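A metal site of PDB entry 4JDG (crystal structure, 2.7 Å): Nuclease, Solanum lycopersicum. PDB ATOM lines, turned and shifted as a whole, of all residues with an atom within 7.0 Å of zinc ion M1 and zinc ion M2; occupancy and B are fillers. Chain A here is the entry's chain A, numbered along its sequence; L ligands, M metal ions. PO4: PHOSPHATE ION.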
ATOM      1  N   TRP A   1      -1.348   4.052 -21.946  1.00  0.00           N
ATOM      2  CA  TRP A   1       0.014   4.211 -22.467  1.00  0.00           C
ATOM      3  C   TRP A   1       0.830   2.954 -22.183  1.00  0.00           C
ATOM      4  O   TRP A   1       0.545   2.230 -21.241  1.00  0.00           O
ATOM      5  CB  TRP A   1       0.701   5.380 -21.788  1.00  0.00           C
ATOM      6  CG  TRP A   1       0.084   6.771 -21.954  1.00  0.00           C
ATOM      7  CD1 TRP A   1      -0.300   7.604 -20.940  1.00  0.00           C
ATOM      8  CD2 TRP A   1      -0.133   7.500 -23.169  1.00  0.00           C
ATOM      9  NE1 TRP A   1      -0.756   8.787 -21.440  1.00  0.00           N
ATOM     10  CE2 TRP A   1      -0.663   8.756 -22.809  1.00  0.00           C
ATOM     11  CE3 TRP A   1       0.072   7.219 -24.521  1.00  0.00           C
ATOM     12  CZ2 TRP A   1      -1.005   9.722 -23.758  1.00  0.00           C
ATOM     13  CZ3 TRP A   1      -0.266   8.190 -25.462  1.00  0.00           C
ATOM     14  CH2 TRP A   1      -0.804   9.415 -25.076  1.00  0.00           C
ATOM     15  N   SER A   2       1.859   2.708 -23.000  1.00  0.00           N
ATOM     16  CA  SER A   2       2.845   1.686 -22.733  1.00  0.00           C
ATOM     17  C   SER A   2       3.912   2.320 -21.880  1.00  0.00           C
ATOM     18  O   SER A   2       3.767   3.475 -21.489  1.00  0.00           O
ATOM     19  CB  SER A   2       3.412   1.165 -24.026  1.00  0.00           C
ATOM     20  OG  SER A   2       2.347   0.671 -24.816  1.00  0.00           O
ATOM     21  N   LYS A   3       4.981   1.577 -21.598  1.00  0.00           N
ATOM     22  CA  LYS A   3       6.040   2.067 -20.707  1.00  0.00           C
ATOM     23  C   LYS A   3       6.238   3.559 -20.849  1.00  0.00           C
ATOM     24  O   LYS A   3       6.167   4.321 -19.865  1.00  0.00           O
ATOM     25  CB  LYS A   3       7.375   1.371 -21.008  1.00  0.00           C
ATOM     26  CG  LYS A   3       7.330  -0.145 -20.854  1.00  0.00           C
ATOM     27  CD  LYS A   3       8.492  -0.645 -20.003  1.00  0.00           C
ATOM     28  CE  LYS A   3       8.095  -1.872 -19.211  1.00  0.00           C
ATOM     29  NZ  LYS A   3       9.082  -2.286 -18.188  1.00  0.00           N
ATOM     30  N   GLY A   5       4.728   6.388 -22.280  1.00  0.00           N
ATOM     31  CA  GLY A   5       3.741   7.406 -21.875  1.00  0.00           C
ATOM     32  C   GLY A   5       3.651   7.543 -20.367  1.00  0.00           C
ATOM     33  O   GLY A   5       3.715   8.658 -19.811  1.00  0.00           O
ATOM     34  N   HIS A   6       3.552   6.407 -19.684  1.00  0.00           N
ATOM     35  CA  HIS A   6       3.502   6.444 -18.236  1.00  0.00           C
ATOM     36  C   HIS A   6       4.749   7.067 -17.622  1.00  0.00           C
ATOM     37  O   HIS A   6       4.640   7.894 -16.717  1.00  0.00           O
ATOM     38  CB  HIS A   6       3.249   5.060 -17.683  1.00  0.00           C
ATOM     39  CG  HIS A   6       1.906   4.534 -18.043  1.00  0.00           C
ATOM     40  ND1 HIS A   6       0.745   5.049 -17.499  1.00  0.00           N
ATOM     41  CD2 HIS A   6       1.514   3.572 -18.910  1.00  0.00           C
ATOM     42  CE1 HIS A   6      -0.292   4.420 -18.025  1.00  0.00           C
ATOM     43  NE2 HIS A   6       0.155   3.515 -18.863  1.00  0.00           N
ATOM     44  N   CYS A  41       5.377   3.283 -12.374  1.00  0.00           N
ATOM     45  CA  CYS A  41       4.074   3.628 -12.985  1.00  0.00           C
ATOM     46  C   CYS A  41       3.513   2.551 -13.907  1.00  0.00           C
ATOM     47  O   CYS A  41       2.335   2.562 -14.195  1.00  0.00           O
ATOM     48  CB  CYS A  41       4.139   4.981 -13.719  1.00  0.00           C
ATOM     49  SG  CYS A  41       4.116   6.337 -12.520  1.00  0.00           S
ATOM     50  N   VAL A  42       4.348   1.649 -14.401  1.00  0.00           N
ATOM     51  CA  VAL A  42       3.863   0.565 -15.266  1.00  0.00           C
ATOM     52  C   VAL A  42       3.328  -0.592 -14.419  1.00  0.00           C
ATOM     53  O   VAL A  42       2.547  -1.393 -14.888  1.00  0.00           O
ATOM     54  CB  VAL A  42       4.970   0.090 -16.249  1.00  0.00           C
ATOM     55  CG1 VAL A  42       4.487  -1.036 -17.139  1.00  0.00           C
ATOM     56  CG2 VAL A  42       5.367   1.241 -17.135  1.00  0.00           C
ATOM     57  N   PRO A  44       0.967  -1.466 -12.538  1.00  0.00           N
ATOM     58  CA  PRO A  44      -0.379  -2.000 -12.730  1.00  0.00           C
ATOM     59  C   PRO A  44      -0.570  -2.793 -14.000  1.00  0.00           C
ATOM     60  O   PRO A  44      -1.546  -3.527 -14.112  1.00  0.00           O
ATOM     61  CB  PRO A  44      -1.247  -0.744 -12.783  1.00  0.00           C
ATOM     62  CG  PRO A  44      -0.496   0.232 -11.964  1.00  0.00           C
ATOM     63  CD  PRO A  44       0.941  -0.018 -12.271  1.00  0.00           C
ATOM     64  N   ASP A  45       0.314  -2.604 -14.972  1.00  0.00           N
ATOM     65  CA  ASP A  45       0.157  -3.223 -16.289  1.00  0.00           C
ATOM     66  C   ASP A  45       0.736  -4.627 -16.265  1.00  0.00           C
ATOM     67  O   ASP A  45       0.396  -5.460 -17.105  1.00  0.00           O
ATOM     68  CB  ASP A  45       0.887  -2.395 -17.364  1.00  0.00           C
ATOM     69  CG  ASP A  45      -0.044  -1.701 -18.331  1.00  0.00           C
ATOM     70  OD1 ASP A  45      -1.227  -2.067 -18.463  1.00  0.00           O
ATOM     71  OD2 ASP A  45       0.445  -0.795 -19.032  1.00  0.00           O
ATOM     72  N   ARG A  48      -1.885  -6.726 -14.058  1.00  0.00           N
ATOM     73  CA  ARG A  48      -3.086  -6.850 -14.883  1.00  0.00           C
ATOM     74  C   ARG A  48      -3.416  -8.318 -15.234  1.00  0.00           C
ATOM     75  O   ARG A  48      -4.581  -8.663 -15.443  1.00  0.00           O
ATOM     76  CB  ARG A  48      -2.795  -6.044 -16.167  1.00  0.00           C
ATOM     77  CG  ARG A  48      -3.910  -5.869 -17.180  1.00  0.00           C
ATOM     78  CD  ARG A  48      -3.352  -5.161 -18.424  1.00  0.00           C
ATOM     79  NE  ARG A  48      -4.190  -4.065 -18.893  1.00  0.00           N
ATOM     80  CZ  ARG A  48      -5.421  -4.210 -19.391  1.00  0.00           C
ATOM     81  NH1 ARG A  48      -5.994  -5.409 -19.458  1.00  0.00           N
ATOM     82  NH2 ARG A  48      -6.102  -3.146 -19.805  1.00  0.00           N
ATOM     83  N   LEU A  59     -10.333  -1.670 -15.193  1.00  0.00           N
ATOM     84  CA  LEU A  59     -10.040  -0.335 -14.663  1.00  0.00           C
ATOM     85  C   LEU A  59      -9.070   0.461 -15.528  1.00  0.00           C
ATOM     86  O   LEU A  59      -8.640   1.545 -15.142  1.00  0.00           O
ATOM     87  CB  LEU A  59      -9.457  -0.444 -13.226  1.00  0.00           C
ATOM     88  CG  LEU A  59     -10.234  -1.131 -12.102  1.00  0.00           C
ATOM     89  CD1 LEU A  59      -9.541  -0.947 -10.755  1.00  0.00           C
ATOM     90  CD2 LEU A  59     -11.628  -0.559 -12.017  1.00  0.00           C
ATOM     91  N   HIS A  60      -8.647  -0.063 -16.658  1.00  0.00           N
ATOM     92  CA  HIS A  60      -7.653   0.660 -17.473  1.00  0.00           C
ATOM     93  C   HIS A  60      -8.313   1.545 -18.510  1.00  0.00           C
ATOM     94  O   HIS A  60      -7.694   2.498 -19.020  1.00  0.00           O
ATOM     95  CB  HIS A  60      -6.716  -0.343 -18.155  1.00  0.00           C
ATOM     96  CG  HIS A  60      -5.722  -0.926 -17.206  1.00  0.00           C
ATOM     97  ND1 HIS A  60      -4.365  -0.778 -17.368  1.00  0.00           N
ATOM     98  CD2 HIS A  60      -5.881  -1.632 -16.065  1.00  0.00           C
ATOM     99  CE1 HIS A  60      -3.735  -1.361 -16.365  1.00  0.00           C
ATOM    100  NE2 HIS A  60      -4.638  -1.899 -15.568  1.00  0.00           N
ATOM    101  N   PHE A  61      -9.586   1.249 -18.800  1.00  0.00           N
ATOM    102  CA  PHE A  61     -10.270   1.860 -19.901  1.00  0.00           C
ATOM    103  C   PHE A  61     -11.737   2.182 -19.629  1.00  0.00           C
ATOM    104  O   PHE A  61     -12.256   1.985 -18.507  1.00  0.00           O
ATOM    105  CB  PHE A  61     -10.157   0.939 -21.105  1.00  0.00           C
ATOM    106  CG  PHE A  61     -10.680  -0.429 -20.855  1.00  0.00           C
ATOM    107  CD1 PHE A  61      -9.860  -1.416 -20.332  1.00  0.00           C
ATOM    108  CD2 PHE A  61     -11.981  -0.769 -21.192  1.00  0.00           C
ATOM    109  CE1 PHE A  61     -10.349  -2.706 -20.128  1.00  0.00           C
ATOM    110  CE2 PHE A  61     -12.470  -2.059 -20.988  1.00  0.00           C
ATOM    111  CZ  PHE A  61     -11.661  -3.015 -20.454  1.00  0.00           C
ATOM    112  N   HIS A 122      -0.822   5.579 -12.510  1.00  0.00           N
ATOM    113  CA  HIS A 122      -0.940   4.853 -13.774  1.00  0.00           C
ATOM    114  C   HIS A 122      -2.228   5.187 -14.507  1.00  0.00           C
ATOM    115  O   HIS A 122      -2.200   5.499 -15.689  1.00  0.00           O
ATOM    116  CB  HIS A 122      -0.911   3.354 -13.526  1.00  0.00           C
ATOM    117  CG  HIS A 122      -1.040   2.554 -14.773  1.00  0.00           C
ATOM    118  ND1 HIS A 122       0.052   2.168 -15.515  1.00  0.00           N
ATOM    119  CD2 HIS A 122      -2.141   2.127 -15.443  1.00  0.00           C
ATOM    120  CE1 HIS A 122      -0.372   1.511 -16.590  1.00  0.00           C
ATOM    121  NE2 HIS A 122      -1.691   1.467 -16.561  1.00  0.00           N
ATOM    122  N   PHE A 123      -3.353   5.091 -13.814  1.00  0.00           N
ATOM    123  CA  PHE A 123      -4.680   5.351 -14.407  1.00  0.00           C
ATOM    124  C   PHE A 123      -4.925   6.812 -14.790  1.00  0.00           C
ATOM    125  O   PHE A 123      -5.729   7.117 -15.678  1.00  0.00           O
ATOM    126  CB  PHE A 123      -5.771   4.884 -13.461  1.00  0.00           C
ATOM    127  CG  PHE A 123      -5.765   3.397 -13.195  1.00  0.00           C
ATOM    128  CD1 PHE A 123      -5.809   2.513 -14.231  1.00  0.00           C
ATOM    129  CD2 PHE A 123      -5.801   2.908 -11.899  1.00  0.00           C
ATOM    130  CE1 PHE A 123      -5.821   1.147 -13.999  1.00  0.00           C
ATOM    131  CE2 PHE A 123      -5.817   1.550 -11.657  1.00  0.00           C
ATOM    132  CZ  PHE A 123      -5.825   0.666 -12.712  1.00  0.00           C
ATOM    133  N   GLY A 125      -2.657   8.535 -16.271  1.00  0.00           N
ATOM    134  CA  GLY A 125      -2.085   8.487 -17.614  1.00  0.00           C
ATOM    135  C   GLY A 125      -2.977   7.754 -18.603  1.00  0.00           C
ATOM    136  O   GLY A 125      -3.070   8.173 -19.765  1.00  0.00           O
ATOM    137  N   ASP A 126      -3.634   6.666 -18.165  1.00  0.00           N
ATOM    138  CA  ASP A 126      -4.471   5.879 -19.093  1.00  0.00           C
ATOM    139  C   ASP A 126      -5.695   6.674 -19.579  1.00  0.00           C
ATOM    140  O   ASP A 126      -6.055   6.592 -20.754  1.00  0.00           O
ATOM    141  CB  ASP A 126      -4.928   4.545 -18.475  1.00  0.00           C
ATOM    142  CG  ASP A 126      -3.963   3.372 -18.786  1.00  0.00           C
ATOM    143  OD1 ASP A 126      -2.885   3.588 -19.336  1.00  0.00           O
ATOM    144  OD2 ASP A 126      -4.307   2.216 -18.462  1.00  0.00           O
ATOM    145  N   GLN A 129      -4.954   8.842 -22.581  1.00  0.00           N
ATOM    146  CA  GLN A 129      -4.692   8.131 -23.840  1.00  0.00           C
ATOM    147  C   GLN A 129      -6.029   8.031 -24.552  1.00  0.00           C
ATOM    148  O   GLN A 129      -6.868   7.245 -24.141  1.00  0.00           O
ATOM    149  CB  GLN A 129      -4.112   6.732 -23.593  1.00  0.00           C
ATOM    150  CG  GLN A 129      -3.185   6.243 -24.694  1.00  0.00           C
ATOM    151  CD  GLN A 129      -3.918   5.637 -25.859  1.00  0.00           C
ATOM    152  OE1 GLN A 129      -4.842   6.219 -26.405  1.00  0.00           O
ATOM    153  NE2 GLN A 129      -3.507   4.434 -26.244  1.00  0.00           N
ATOM    154  N   HIS A 132      -8.136   4.946 -24.838  1.00  0.00           N
ATOM    155  CA  HIS A 132      -8.620   4.280 -23.625  1.00  0.00           C
ATOM    156  C   HIS A 132     -10.078   4.588 -23.321  1.00  0.00           C
ATOM    157  O   HIS A 132     -10.676   3.998 -22.417  1.00  0.00           O
ATOM    158  CB  HIS A 132      -7.723   4.606 -22.435  1.00  0.00           C
ATOM    159  CG  HIS A 132      -6.525   3.723 -22.382  1.00  0.00           C
ATOM    160  ND1 HIS A 132      -6.308   2.833 -21.350  1.00  0.00           N
ATOM    161  CD2 HIS A 132      -5.550   3.498 -23.292  1.00  0.00           C
ATOM    162  CE1 HIS A 132      -5.216   2.150 -21.605  1.00  0.00           C
ATOM    163  NE2 HIS A 132      -4.744   2.525 -22.784  1.00  0.00           N
ATOM    164  N   ASP A 160      -0.797   4.020 -27.974  1.00  0.00           N
ATOM    165  CA  ASP A 160      -0.086   3.591 -26.747  1.00  0.00           C
ATOM    166  C   ASP A 160       1.428   3.712 -26.885  1.00  0.00           C
ATOM    167  O   ASP A 160       2.131   3.921 -25.895  1.00  0.00           O
ATOM    168  CB  ASP A 160      -0.414   2.138 -26.399  1.00  0.00           C
ATOM    169  CG  ASP A 160      -1.529   2.005 -25.405  1.00  0.00           C
ATOM    170  OD1 ASP A 160      -1.269   2.102 -24.185  1.00  0.00           O
ATOM    171  OD2 ASP A 160      -2.673   1.788 -25.835  1.00  0.00           O
HETATM  172  P   PO4 L   1      -2.153   0.430 -21.032  1.00  0.00           P
HETATM  173  O1  PO4 L   1      -2.297   1.820 -21.703  1.00  0.00           O
HETATM  174  O2  PO4 L   1      -1.835  -0.628 -22.108  1.00  0.00           O
HETATM  175  O3  PO4 L   1      -1.012   0.525 -20.033  1.00  0.00           O
HETATM  176  O4  PO4 L   1      -3.378  -0.018 -20.213  1.00  0.00           O
HETATM  177 ZN    ZN M   1      -1.088   2.780 -20.071  1.00  0.00          ZN
HETATM  178 ZN    ZN M   2      -2.846   0.607 -18.172  1.00  0.00          ZN
HETATM  179 ZN    ZN M   3      -3.409   0.861 -23.818  1.00  0.00          ZN
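Within 4 Å of zinc ion M1: Trp 1, His 6, His 122 and Asp 126.
Zinc ion M2 is bound by NE2 of His 122 (2.2 Å), OD2 of Asp 126 (2.2 Å), O4 of the ligand (2.2 Å) and ND1 of His 60 (2.2 Å). Slightly farther from zinc ion M2 lies O3 of the ligand (2.6 Å).
Zinc ion M1 is bound by NE2 of His 6 (1.9 Å), O of Trp 1 (2.1 Å), OD1 of Asp 126 (2.1 Å), O1 of the ligand (2.2 Å), O3 of the ligand (2.3 Å) and N of Trp 1 (2.3 Å).
Residues that only touch zinc ion M2: Asp 45 (3.1 Å). Of the 20 residues printed, 4 come within 4 Å of zinc ion M2. The nearest printed residue that does not touch zinc ion M2 is His 6 (4.2 Å).
ND1 of His 6 lies close to O of His 122, at 3.5 Å. The backbone carbonyl oxygen (O) of Gly 125 sits at hydrogen-bond distance from the indole nitrogen (NE1) of Trp 1. A ring nitrogen (ND1) of His 122 sits at hydrogen-bond distance from the backbone carbonyl oxygen (O) of Cys 41 (2.7 Å). The backbone carbonyl oxygen of His 60 sits at hydrogen-bond distance from a ring nitrogen (ND1) of His 132, 2.7 Å away. The guanidinium group (NE) of Arg 48 lies within salt-bridge range of the side-chain carboxylate (OD1) of Asp 45 (3.6 Å).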
